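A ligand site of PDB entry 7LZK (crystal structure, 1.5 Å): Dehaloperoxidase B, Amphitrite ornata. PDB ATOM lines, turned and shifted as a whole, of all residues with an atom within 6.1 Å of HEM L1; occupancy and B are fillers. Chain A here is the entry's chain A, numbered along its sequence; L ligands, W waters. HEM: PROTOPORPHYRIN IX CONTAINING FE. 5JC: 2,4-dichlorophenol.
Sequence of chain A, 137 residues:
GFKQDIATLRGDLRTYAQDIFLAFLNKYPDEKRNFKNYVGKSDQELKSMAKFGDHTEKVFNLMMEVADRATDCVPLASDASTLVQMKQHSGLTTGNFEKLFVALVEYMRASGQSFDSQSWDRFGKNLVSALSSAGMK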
ATOM      1  N   PHE A  24      17.161 -33.574   5.350  1.00  0.00           N
ATOM      2  CA  PHE A  24      16.804 -32.954   6.621  1.00  0.00           C
ATOM      3  C   PHE A  24      15.290 -32.945   6.834  1.00  0.00           C
ATOM      4  O   PHE A  24      14.804 -33.374   7.893  1.00  0.00           O
ATOM      5  CB  PHE A  24      17.402 -31.537   6.622  1.00  0.00           C
ATOM      6  CG  PHE A  24      16.918 -30.635   7.719  1.00  0.00           C
ATOM      7  CD1 PHE A  24      17.127 -30.947   9.059  1.00  0.00           C
ATOM      8  CD2 PHE A  24      16.314 -29.429   7.401  1.00  0.00           C
ATOM      9  CE1 PHE A  24      16.692 -30.082  10.074  1.00  0.00           C
ATOM     10  CE2 PHE A  24      15.874 -28.550   8.419  1.00  0.00           C
ATOM     11  CZ  PHE A  24      16.064 -28.881   9.742  1.00  0.00           C
ATOM     12  N   GLU A  31      10.292 -30.253  11.126  1.00  0.00           N
ATOM     13  CA  GLU A  31      11.002 -29.050  10.721  1.00  0.00           C
ATOM     14  C   GLU A  31      10.337 -28.322   9.560  1.00  0.00           C
ATOM     15  O   GLU A  31      10.664 -27.155   9.326  1.00  0.00           O
ATOM     16  CB  GLU A  31      12.462 -29.399  10.385  1.00  0.00           C
ATOM     17  CG  GLU A  31      13.258 -29.899  11.586  1.00  0.00           C
ATOM     18  CD  GLU A  31      13.538 -28.797  12.594  1.00  0.00           C
ATOM     19  OE1 GLU A  31      13.474 -29.054  13.817  1.00  0.00           O
ATOM     20  OE2 GLU A  31      13.806 -27.654  12.170  1.00  0.00           O
ATOM     21  N   ASN A  34       8.662 -24.645   9.854  1.00  0.00           N
ATOM     22  CA  ASN A  34       9.417 -23.406   9.717  1.00  0.00           C
ATOM     23  C   ASN A  34       9.335 -22.818   8.316  1.00  0.00           C
ATOM     24  O   ASN A  34       9.818 -21.700   8.107  1.00  0.00           O
ATOM     25  CB  ASN A  34      10.898 -23.633  10.055  1.00  0.00           C
ATOM     26  CG  ASN A  34      11.100 -24.070  11.487  1.00  0.00           C
ATOM     27  OD1 ASN A  34      10.976 -23.269  12.411  1.00  0.00           O
ATOM     28  ND2 ASN A  34      11.440 -25.347  11.684  1.00  0.00           N
ATOM     29  N   PHE A  35       8.742 -23.523   7.363  1.00  0.00           N
ATOM     30  CA  PHE A  35       8.727 -23.096   5.973  1.00  0.00           C
ATOM     31  C   PHE A  35       7.287 -22.993   5.471  1.00  0.00           C
ATOM     32  O   PHE A  35       6.362 -23.560   6.065  1.00  0.00           O
ATOM     33  CB  PHE A  35       9.549 -24.050   5.106  1.00  0.00           C
ATOM     34  CG  PHE A  35      10.979 -24.204   5.573  1.00  0.00           C
ATOM     35  CD1 PHE A  35      11.325 -25.189   6.486  1.00  0.00           C
ATOM     36  CD2 PHE A  35      11.964 -23.343   5.113  1.00  0.00           C
ATOM     37  CE1 PHE A  35      12.620 -25.318   6.930  1.00  0.00           C
ATOM     38  CE2 PHE A  35      13.263 -23.469   5.549  1.00  0.00           C
ATOM     39  CZ  PHE A  35      13.597 -24.452   6.467  1.00  0.00           C
ATOM     40  N   TYR A  38       5.439 -26.171   2.356  1.00  0.00           N
ATOM     41  CA  TYR A  38       6.163 -27.416   2.111  1.00  0.00           C
ATOM     42  C   TYR A  38       5.372 -28.649   2.524  1.00  0.00           C
ATOM     43  O   TYR A  38       5.755 -29.772   2.165  1.00  0.00           O
ATOM     44  CB  TYR A  38       7.527 -27.409   2.824  1.00  0.00           C
ATOM     45  CG  TYR A  38       8.573 -26.505   2.199  1.00  0.00           C
ATOM     46  CD1 TYR A  38       8.277 -25.725   1.086  1.00  0.00           C
ATOM     47  CD2 TYR A  38       9.850 -26.428   2.730  1.00  0.00           C
ATOM     48  CE1 TYR A  38       9.237 -24.892   0.522  1.00  0.00           C
ATOM     49  CE2 TYR A  38      10.815 -25.603   2.177  1.00  0.00           C
ATOM     50  CZ  TYR A  38      10.506 -24.837   1.077  1.00  0.00           C
ATOM     51  OH  TYR A  38      11.467 -24.020   0.519  1.00  0.00           O
ATOM     52  N   LYS A  51      10.708 -20.504  -5.721  1.00  0.00           N
ATOM     53  CA  LYS A  51      11.585 -20.377  -4.551  1.00  0.00           C
ATOM     54  C   LYS A  51      12.393 -21.593  -4.076  1.00  0.00           C
ATOM     55  O   LYS A  51      13.490 -21.380  -3.551  1.00  0.00           O
ATOM     56  CB  LYS A  51      10.791 -19.787  -3.378  1.00  0.00           C
ATOM     57  N   ASP A  54      15.929 -21.842  -5.491  1.00  0.00           N
ATOM     58  CA  ASP A  54      16.617 -20.580  -5.208  1.00  0.00           C
ATOM     59  C   ASP A  54      16.967 -20.482  -3.724  1.00  0.00           C
ATOM     60  O   ASP A  54      18.110 -20.153  -3.369  1.00  0.00           O
ATOM     61  CB  ASP A  54      15.748 -19.408  -5.645  1.00  0.00           C
ATOM     62  CG  ASP A  54      16.401 -18.056  -5.383  1.00  0.00           C
ATOM     63  OD1 ASP A  54      17.310 -17.675  -6.156  1.00  0.00           O
ATOM     64  OD2 ASP A  54      16.007 -17.364  -4.421  1.00  0.00           O
ATOM     65  N   HIS A  55      16.005 -20.808  -2.853  1.00  0.00           N
ATOM     66  CA  HIS A  55      16.240 -20.796  -1.409  1.00  0.00           C
ATOM     67  C   HIS A  55      17.309 -21.800  -1.011  1.00  0.00           C
ATOM     68  O   HIS A  55      18.295 -21.447  -0.340  1.00  0.00           O
ATOM     69  CB  HIS A  55      14.938 -21.120  -0.658  1.00  0.00           C
ATOM     70  CG  HIS A  55      15.145 -21.576   0.758  1.00  0.00           C
ATOM     71  ND1 HIS A  55      15.342 -20.692   1.800  1.00  0.00           N
ATOM     72  CD2 HIS A  55      15.187 -22.807   1.304  1.00  0.00           C
ATOM     73  CE1 HIS A  55      15.495 -21.365   2.926  1.00  0.00           C
ATOM     74  NE2 HIS A  55      15.404 -22.654   2.648  1.00  0.00           N
ATOM     75  N   LYS A  58      20.760 -20.665  -2.002  1.00  0.00           N
ATOM     76  CA  LYS A  58      21.300 -19.543  -1.233  1.00  0.00           C
ATOM     77  C   LYS A  58      21.720 -19.975   0.168  1.00  0.00           C
ATOM     78  O   LYS A  58      22.774 -19.551   0.665  1.00  0.00           O
ATOM     79  CB  LYS A  58      20.283 -18.394  -1.191  1.00  0.00           C
ATOM     80  CG  LYS A  58      20.261 -17.617  -2.472  1.00  0.00           C
ATOM     81  CD  LYS A  58      19.114 -16.642  -2.521  1.00  0.00           C
ATOM     82  CE  LYS A  58      19.128 -15.828  -3.807  1.00  0.00           C
ATOM     83  NZ  LYS A  58      17.853 -15.063  -3.993  1.00  0.00           N
ATOM     84  N   VAL A  59      20.950 -20.854   0.811  1.00  0.00           N
ATOM     85  CA  VAL A  59      21.347 -21.368   2.114  1.00  0.00           C
ATOM     86  C   VAL A  59      22.655 -22.135   1.999  1.00  0.00           C
ATOM     87  O   VAL A  59      23.598 -21.939   2.782  1.00  0.00           O
ATOM     88  CB  VAL A  59      20.237 -22.262   2.688  1.00  0.00           C
ATOM     89  CG1 VAL A  59      20.726 -22.951   3.962  1.00  0.00           C
ATOM     90  CG2 VAL A  59      18.964 -21.469   2.946  1.00  0.00           C
ATOM     91  N   PHE A  60      22.711 -23.050   1.025  1.00  0.00           N
ATOM     92  CA  PHE A  60      23.885 -23.901   0.861  1.00  0.00           C
ATOM     93  C   PHE A  60      25.112 -23.095   0.454  1.00  0.00           C
ATOM     94  O   PHE A  60      26.228 -23.393   0.902  1.00  0.00           O
ATOM     95  CB  PHE A  60      23.572 -24.972  -0.176  1.00  0.00           C
ATOM     96  CG  PHE A  60      24.415 -26.194  -0.061  1.00  0.00           C
ATOM     97  CD1 PHE A  60      24.333 -27.017   1.059  1.00  0.00           C
ATOM     98  CD2 PHE A  60      25.294 -26.539  -1.082  1.00  0.00           C
ATOM     99  CE1 PHE A  60      25.120 -28.143   1.157  1.00  0.00           C
ATOM    100  CE2 PHE A  60      26.086 -27.661  -0.992  1.00  0.00           C
ATOM    101  CZ  PHE A  60      25.995 -28.479   0.126  1.00  0.00           C
ATOM    102  N   LEU A  62      25.857 -20.127   1.415  1.00  0.00           N
ATOM    103  CA  LEU A  62      26.410 -19.529   2.627  1.00  0.00           C
ATOM    104  C   LEU A  62      26.999 -20.583   3.553  1.00  0.00           C
ATOM    105  O   LEU A  62      28.061 -20.357   4.147  1.00  0.00           O
ATOM    106  CB  LEU A  62      25.355 -18.688   3.337  1.00  0.00           C
ATOM    107  CG  LEU A  62      25.882 -17.928   4.569  1.00  0.00           C
ATOM    108  CD1 LEU A  62      27.121 -17.085   4.240  1.00  0.00           C
ATOM    109  CD2 LEU A  62      24.788 -17.060   5.177  1.00  0.00           C
ATOM    110  N   MET A  63      26.345 -21.746   3.672  1.00  0.00           N
ATOM    111  CA  MET A  63      26.937 -22.803   4.494  1.00  0.00           C
ATOM    112  C   MET A  63      28.332 -23.164   4.016  1.00  0.00           C
ATOM    113  O   MET A  63      29.247 -23.354   4.823  1.00  0.00           O
ATOM    114  CB  MET A  63      26.042 -24.036   4.539  1.00  0.00           C
ATOM    115  CG  MET A  63      26.560 -25.087   5.514  1.00  0.00           C
ATOM    116  SD  MET A  63      25.872 -26.715   5.241  1.00  0.00           S
ATOM    117  CE  MET A  63      24.207 -26.468   5.827  1.00  0.00           C
ATOM    118  N   VAL A  66      30.779 -20.458   5.095  1.00  0.00           N
ATOM    119  CA  VAL A  66      31.109 -20.559   6.511  1.00  0.00           C
ATOM    120  C   VAL A  66      32.082 -21.718   6.736  1.00  0.00           C
ATOM    121  O   VAL A  66      33.053 -21.589   7.485  1.00  0.00           O
ATOM    122  CB  VAL A  66      29.810 -20.701   7.351  1.00  0.00           C
ATOM    123  CG1 VAL A  66      30.131 -20.930   8.822  1.00  0.00           C
ATOM    124  CG2 VAL A  66      28.911 -19.463   7.167  1.00  0.00           C
ATOM    125  N   LEU A  83      24.417 -15.348  11.287  1.00  0.00           N
ATOM    126  CA  LEU A  83      23.319 -16.308  11.235  1.00  0.00           C
ATOM    127  C   LEU A  83      22.314 -16.080  12.363  1.00  0.00           C
ATOM    128  O   LEU A  83      21.108 -16.246  12.163  1.00  0.00           O
ATOM    129  CB  LEU A  83      23.869 -17.737  11.295  1.00  0.00           C
ATOM    130  CG  LEU A  83      24.739 -18.169  10.111  1.00  0.00           C
ATOM    131  CD1 LEU A  83      25.399 -19.522  10.381  1.00  0.00           C
ATOM    132  CD2 LEU A  83      23.892 -18.232   8.849  1.00  0.00           C
ATOM    133  N   MET A  86      20.077 -12.740  11.451  1.00  0.00           N
ATOM    134  CA  MET A  86      19.208 -12.740  10.271  1.00  0.00           C
ATOM    135  C   MET A  86      17.747 -12.782  10.703  1.00  0.00           C
ATOM    136  O   MET A  86      17.347 -13.614  11.510  1.00  0.00           O
ATOM    137  CB  MET A  86      19.508 -13.954   9.406  1.00  0.00           C
ATOM    138  CG  MET A  86      20.738 -13.811   8.555  1.00  0.00           C
ATOM    139  SD  MET A  86      21.173 -15.372   7.775  1.00  0.00           S
ATOM    140  CE  MET A  86      19.663 -15.722   6.867  1.00  0.00           C
ATOM    141  N   GLN A  88      15.291 -13.823   9.095  1.00  0.00           N
ATOM    142  CA  GLN A  88      14.679 -15.096   8.728  1.00  0.00           C
ATOM    143  C   GLN A  88      14.948 -16.196   9.749  1.00  0.00           C
ATOM    144  O   GLN A  88      14.295 -17.242   9.688  1.00  0.00           O
ATOM    145  CB  GLN A  88      15.139 -15.526   7.329  1.00  0.00           C
ATOM    146  CG  GLN A  88      14.529 -14.666   6.219  1.00  0.00           C
ATOM    147  CD  GLN A  88      15.313 -14.727   4.912  1.00  0.00           C
ATOM    148  OE1 GLN A  88      16.479 -14.348   4.862  1.00  0.00           O
ATOM    149  NE2 GLN A  88      14.653 -15.183   3.838  1.00  0.00           N
ATOM    150  N   HIS A  89      15.870 -15.966  10.685  1.00  0.00           N
ATOM    151  CA  HIS A  89      16.220 -16.932  11.711  1.00  0.00           C
ATOM    152  C   HIS A  89      15.698 -16.573  13.089  1.00  0.00           C
ATOM    153  O   HIS A  89      16.036 -17.252  14.059  1.00  0.00           O
ATOM    154  CB  HIS A  89      17.747 -17.087  11.781  1.00  0.00           C
ATOM    155  CG  HIS A  89      18.325 -17.808  10.619  1.00  0.00           C
ATOM    156  ND1 HIS A  89      19.674 -17.851  10.359  1.00  0.00           N
ATOM    157  CD2 HIS A  89      17.728 -18.514   9.628  1.00  0.00           C
ATOM    158  CE1 HIS A  89      19.894 -18.556   9.259  1.00  0.00           C
ATOM    159  NE2 HIS A  89      18.724 -18.974   8.800  1.00  0.00           N
ATOM    160  N   LEU A  92      14.353 -19.331  15.756  1.00  0.00           N
ATOM    161  CA  LEU A  92      15.025 -20.625  15.679  1.00  0.00           C
ATOM    162  C   LEU A  92      15.874 -20.841  16.925  1.00  0.00           C
ATOM    163  O   LEU A  92      16.234 -19.900  17.635  1.00  0.00           O
ATOM    164  CB  LEU A  92      15.942 -20.707  14.454  1.00  0.00           C
ATOM    165  CG  LEU A  92      15.312 -20.691  13.058  1.00  0.00           C
ATOM    166  CD1 LEU A  92      16.389 -20.798  11.986  1.00  0.00           C
ATOM    167  CD2 LEU A  92      14.287 -21.807  12.918  1.00  0.00           C
ATOM    168  N   ASN A  96      17.549 -26.633  15.884  1.00  0.00           N
ATOM    169  CA  ASN A  96      17.254 -26.715  14.457  1.00  0.00           C
ATOM    170  C   ASN A  96      18.520 -26.962  13.650  1.00  0.00           C
ATOM    171  O   ASN A  96      18.526 -27.737  12.689  1.00  0.00           O
ATOM    172  CB  ASN A  96      16.598 -25.413  13.971  1.00  0.00           C
ATOM    173  CG  ASN A  96      15.257 -25.114  14.641  1.00  0.00           C
ATOM    174  OD1 ASN A  96      15.174 -24.267  15.520  1.00  0.00           O
ATOM    175  ND2 ASN A  96      14.206 -25.814  14.213  1.00  0.00           N
ATOM    176  N   PHE A  97      19.618 -26.288  14.023  1.00  0.00           N
ATOM    177  CA  PHE A  97      20.874 -26.434  13.306  1.00  0.00           C
ATOM    178  C   PHE A  97      21.536 -27.769  13.607  1.00  0.00           C
ATOM    179  O   PHE A  97      22.122 -28.375  12.712  1.00  0.00           O
ATOM    180  CB  PHE A  97      21.814 -25.269  13.644  1.00  0.00           C
ATOM    181  CG  PHE A  97      21.367 -23.946  13.106  1.00  0.00           C
ATOM    182  CD1 PHE A  97      21.962 -23.407  11.988  1.00  0.00           C
ATOM    183  CD2 PHE A  97      20.337 -23.247  13.721  1.00  0.00           C
ATOM    184  CE1 PHE A  97      21.539 -22.188  11.483  1.00  0.00           C
ATOM    185  CE2 PHE A  97      19.901 -22.042  13.228  1.00  0.00           C
ATOM    186  CZ  PHE A  97      20.508 -21.505  12.103  1.00  0.00           C
ATOM    187  N   LEU A 100      19.931 -30.265  11.439  1.00  0.00           N
ATOM    188  CA  LEU A 100      20.385 -30.153  10.052  1.00  0.00           C
ATOM    189  C   LEU A 100      21.715 -30.868   9.850  1.00  0.00           C
ATOM    190  O   LEU A 100      21.902 -31.574   8.862  1.00  0.00           O
ATOM    191  CB  LEU A 100      20.482 -28.682   9.625  1.00  0.00           C
ATOM    192  CG  LEU A 100      21.165 -28.393   8.286  1.00  0.00           C
ATOM    193  CD1 LEU A 100      20.416 -29.048   7.134  1.00  0.00           C
ATOM    194  CD2 LEU A 100      21.251 -26.892   8.052  1.00  0.00           C
ATOM    195  N   PHE A 101      22.638 -30.707  10.797  1.00  0.00           N
ATOM    196  CA  PHE A 101      23.936 -31.362  10.624  1.00  0.00           C
ATOM    197  C   PHE A 101      23.890 -32.862  10.890  1.00  0.00           C
ATOM    198  O   PHE A 101      24.653 -33.613  10.254  1.00  0.00           O
ATOM    199  CB  PHE A 101      25.020 -30.611  11.391  1.00  0.00           C
ATOM    200  CG  PHE A 101      25.430 -29.340  10.697  1.00  0.00           C
ATOM    201  CD1 PHE A 101      24.808 -28.138  11.001  1.00  0.00           C
ATOM    202  CD2 PHE A 101      26.376 -29.375   9.690  1.00  0.00           C
ATOM    203  CE1 PHE A 101      25.164 -26.982  10.333  1.00  0.00           C
ATOM    204  CE2 PHE A 101      26.732 -28.219   9.023  1.00  0.00           C
ATOM    205  CZ  PHE A 101      26.126 -27.022   9.344  1.00  0.00           C
ATOM    206  N   PHE A 123      32.296 -29.891  12.582  1.00  0.00           N
ATOM    207  CA  PHE A 123      31.925 -28.564  12.129  1.00  0.00           C
ATOM    208  C   PHE A 123      30.528 -28.177  12.628  1.00  0.00           C
ATOM    209  O   PHE A 123      30.316 -27.064  13.126  1.00  0.00           O
ATOM    210  CB  PHE A 123      31.993 -28.516  10.600  1.00  0.00           C
ATOM    211  CG  PHE A 123      31.480 -27.228  10.004  1.00  0.00           C
ATOM    212  CD1 PHE A 123      30.294 -27.202   9.286  1.00  0.00           C
ATOM    213  CD2 PHE A 123      32.182 -26.049  10.183  1.00  0.00           C
ATOM    214  CE1 PHE A 123      29.828 -26.013   8.738  1.00  0.00           C
ATOM    215  CE2 PHE A 123      31.728 -24.857   9.642  1.00  0.00           C
ATOM    216  CZ  PHE A 123      30.551 -24.836   8.926  1.00  0.00           C
ATOM    217  N   LEU A 127      29.698 -25.199  15.071  1.00  0.00           N
ATOM    218  CA  LEU A 127      28.774 -24.141  14.659  1.00  0.00           C
ATOM    219  C   LEU A 127      27.667 -23.947  15.689  1.00  0.00           C
ATOM    220  O   LEU A 127      27.316 -22.805  16.012  1.00  0.00           O
ATOM    221  CB  LEU A 127      28.187 -24.440  13.279  1.00  0.00           C
ATOM    222  CG  LEU A 127      27.311 -23.311  12.729  1.00  0.00           C
ATOM    223  CD1 LEU A 127      28.066 -21.984  12.612  1.00  0.00           C
ATOM    224  CD2 LEU A 127      26.693 -23.698  11.396  1.00  0.00           C
HETATM  225  CHA HEM L   1      16.640 -18.284   5.050  1.00  0.00           C
HETATM  226  CHB HEM L   1      21.374 -19.392   5.588  1.00  0.00           C
HETATM  227  CHC HEM L   1      20.122 -22.935   8.656  1.00  0.00           C
HETATM  228  CHD HEM L   1      15.441 -21.659   8.344  1.00  0.00           C
HETATM  229  C1A HEM L   1      18.015 -18.310   4.868  1.00  0.00           C
HETATM  230  C2A HEM L   1      18.779 -17.576   3.878  1.00  0.00           C
HETATM  231  C3A HEM L   1      20.080 -17.879   4.041  1.00  0.00           C
HETATM  232  C4A HEM L   1      20.192 -18.839   5.116  1.00  0.00           C
HETATM  233  CMA HEM L   1      21.263 -17.333   3.217  1.00  0.00           C
HETATM  234  CAA HEM L   1      18.184 -16.586   2.833  1.00  0.00           C
HETATM  235  CBA HEM L   1      17.620 -17.383   1.651  1.00  0.00           C
HETATM  236  CGA HEM L   1      16.822 -16.530   0.679  1.00  0.00           C
HETATM  237  O1A HEM L   1      16.727 -16.921  -0.501  1.00  0.00           O
HETATM  238  O2A HEM L   1      16.280 -15.469   1.078  1.00  0.00           O
HETATM  239  C1B HEM L   1      21.448 -20.476   6.435  1.00  0.00           C
HETATM  240  C2B HEM L   1      22.649 -21.223   6.755  1.00  0.00           C
HETATM  241  C3B HEM L   1      22.295 -22.220   7.597  1.00  0.00           C
HETATM  242  C4B HEM L   1      20.870 -22.109   7.843  1.00  0.00           C
HETATM  243  CMB HEM L   1      24.032 -20.875   6.158  1.00  0.00           C
HETATM  244  CAB HEM L   1      23.170 -23.296   8.271  1.00  0.00           C
HETATM  245  CBB HEM L   1      24.491 -23.170   8.490  1.00  0.00           C
HETATM  246  C1C HEM L   1      18.744 -22.922   8.820  1.00  0.00           C
HETATM  247  C2C HEM L   1      17.968 -23.861   9.614  1.00  0.00           C
HETATM  248  C3C HEM L   1      16.679 -23.500   9.536  1.00  0.00           C
HETATM  249  C4C HEM L   1      16.595 -22.336   8.688  1.00  0.00           C
HETATM  250  CMC HEM L   1      18.586 -25.032  10.397  1.00  0.00           C
HETATM  251  CAC HEM L   1      15.416 -24.152  10.155  1.00  0.00           C
HETATM  252  CBC HEM L   1      15.362 -25.450  10.465  1.00  0.00           C
HETATM  253  C1D HEM L   1      15.371 -20.617   7.437  1.00  0.00           C
HETATM  254  C2D HEM L   1      14.154 -19.946   7.047  1.00  0.00           C
HETATM  255  C3D HEM L   1      14.475 -19.010   6.144  1.00  0.00           C
HETATM  256  C4D HEM L   1      15.915 -19.073   5.910  1.00  0.00           C
HETATM  257  CMD HEM L   1      12.767 -20.281   7.646  1.00  0.00           C
HETATM  258  CAD HEM L   1      13.515 -18.032   5.428  1.00  0.00           C
HETATM  259  CBD HEM L   1      12.401 -18.765   4.676  1.00  0.00           C
HETATM  260  CGD HEM L   1      12.654 -18.669   3.196  1.00  0.00           C
HETATM  261  O1D HEM L   1      13.828 -18.852   2.777  1.00  0.00           O
HETATM  262  O2D HEM L   1      11.666 -18.432   2.451  1.00  0.00           O
HETATM  263  NA  HEM L   1      18.907 -19.079   5.600  1.00  0.00           N
HETATM  264  NB  HEM L   1      20.381 -21.040   7.112  1.00  0.00           N
HETATM  265  NC  HEM L   1      17.879 -22.009   8.269  1.00  0.00           N
HETATM  266  ND  HEM L   1      16.427 -20.066   6.726  1.00  0.00           N
HETATM  267 FE   HEM L   1      18.420 -20.375   7.125  1.00  0.00          FE
HETATM  268 CL1  5JC L   2      17.707 -25.413   6.666  1.00  0.00          CL
HETATM  269  CAI 5JC L   2      18.229 -25.558   5.024  1.00  0.00           C
HETATM  270  CAF 5JC L   2      19.285 -26.388   4.680  1.00  0.00           C
HETATM  271  CAH 5JC L   2      19.678 -26.462   3.362  1.00  0.00           C
HETATM  272 CL2  5JC L   2      21.001 -27.503   2.936  1.00  0.00          CL
HETATM  273  CAE 5JC L   2      19.018 -25.714   2.398  1.00  0.00           C
HETATM  274  CAD 5JC L   2      17.959 -24.891   2.737  1.00  0.00           C
HETATM  275  CAG 5JC L   2      17.578 -24.815   4.062  1.00  0.00           C
HETATM  276  OAA 5JC L   2      16.516 -23.984   4.474  1.00  0.00           O
HETATM  277  O   HOH W   1      18.220 -13.118   2.718  1.00  0.00           O
HETATM  278  O   HOH W   2      10.351 -19.667   9.756  1.00  0.00           O
HETATM  279  O   HOH W   3       9.495 -20.770   3.242  1.00  0.00           O
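The backbone carbonyl oxygen of Glu 31 sits at hydrogen-bond distance from the side-chain amide nitrogen of Asn 34, at 3.1 Å. OE2 of Glu 31 sits at hydrogen-bond distance from ND2 of Asn 96 (2.8 Å). The side-chain carboxylate of Asp 54 is in salt-bridge range of the side-chain amino group of Lys 58 (3.0 Å). ND1 of His 89 sits at hydrogen-bond distance from O of Leu 83 (2.8 Å).
A ring nitrogen (NE2) of His 55 sits at hydrogen-bond distance from an oxygen (OAA) of 5JC L2 (2.5 Å). O2A of HEM L1 lies within hydrogen-bond range of NE2 of Gln 88 (3.2 Å). FE of HEM L1 is bound by NE2 of His 89 (2.2 Å). A ring nitrogen (ND1) of His 55 sits at hydrogen-bond distance from an oxygen (O1D) of HEM L1 (2.6 Å).
Water W1 bridges OE1 of Gln 88 and O2A of HEM L1.
Phe 24 touches HEM L1 (CZ to CBC, 3.6 Å). Glu 31 touches HEM L1 (OE2 to CBC, 3.2 Å). O of Asn 34 touches CMD of HEM L1, at 3.3 Å. Phe 35 touches HEM L1 (CZ to CHD, 3.8 Å). Lys 58 touches HEM L1 (CD to O1A, 3.1 Å). Val 59 touches HEM L1 (O to CMB, 3.6 Å). Leu 62 touches HEM L1. Met 63 touches HEM L1. Leu 83 touches HEM L1. Met 86 touches HEM L1. Leu 92 touches HEM L1 (CD1 to C4C, 3.6 Å). O of Asn 96 touches CMC of HEM L1, at 3.5 Å. Phe 97 touches HEM L1. CD2 of Leu 127 touches CBB of HEM L1 (3.7 Å). Hydrophobic or aromatic side chains within 4 Å of HEM L1: Phe 24, Phe 35, His 55, Val 59, Leu 62, Leu 83, Met 86, His 89, Leu 92, Phe 97 and Leu 127. Within 4 Å of HEM L1: Phe 24, Glu 31, Asn 34, Phe 35, His 55, Lys 58, Val 59, Leu 62, Met 63, Leu 83, Met 86, Gln 88, His 89, Leu 92, Asn 96, Phe 97 and Leu 127.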
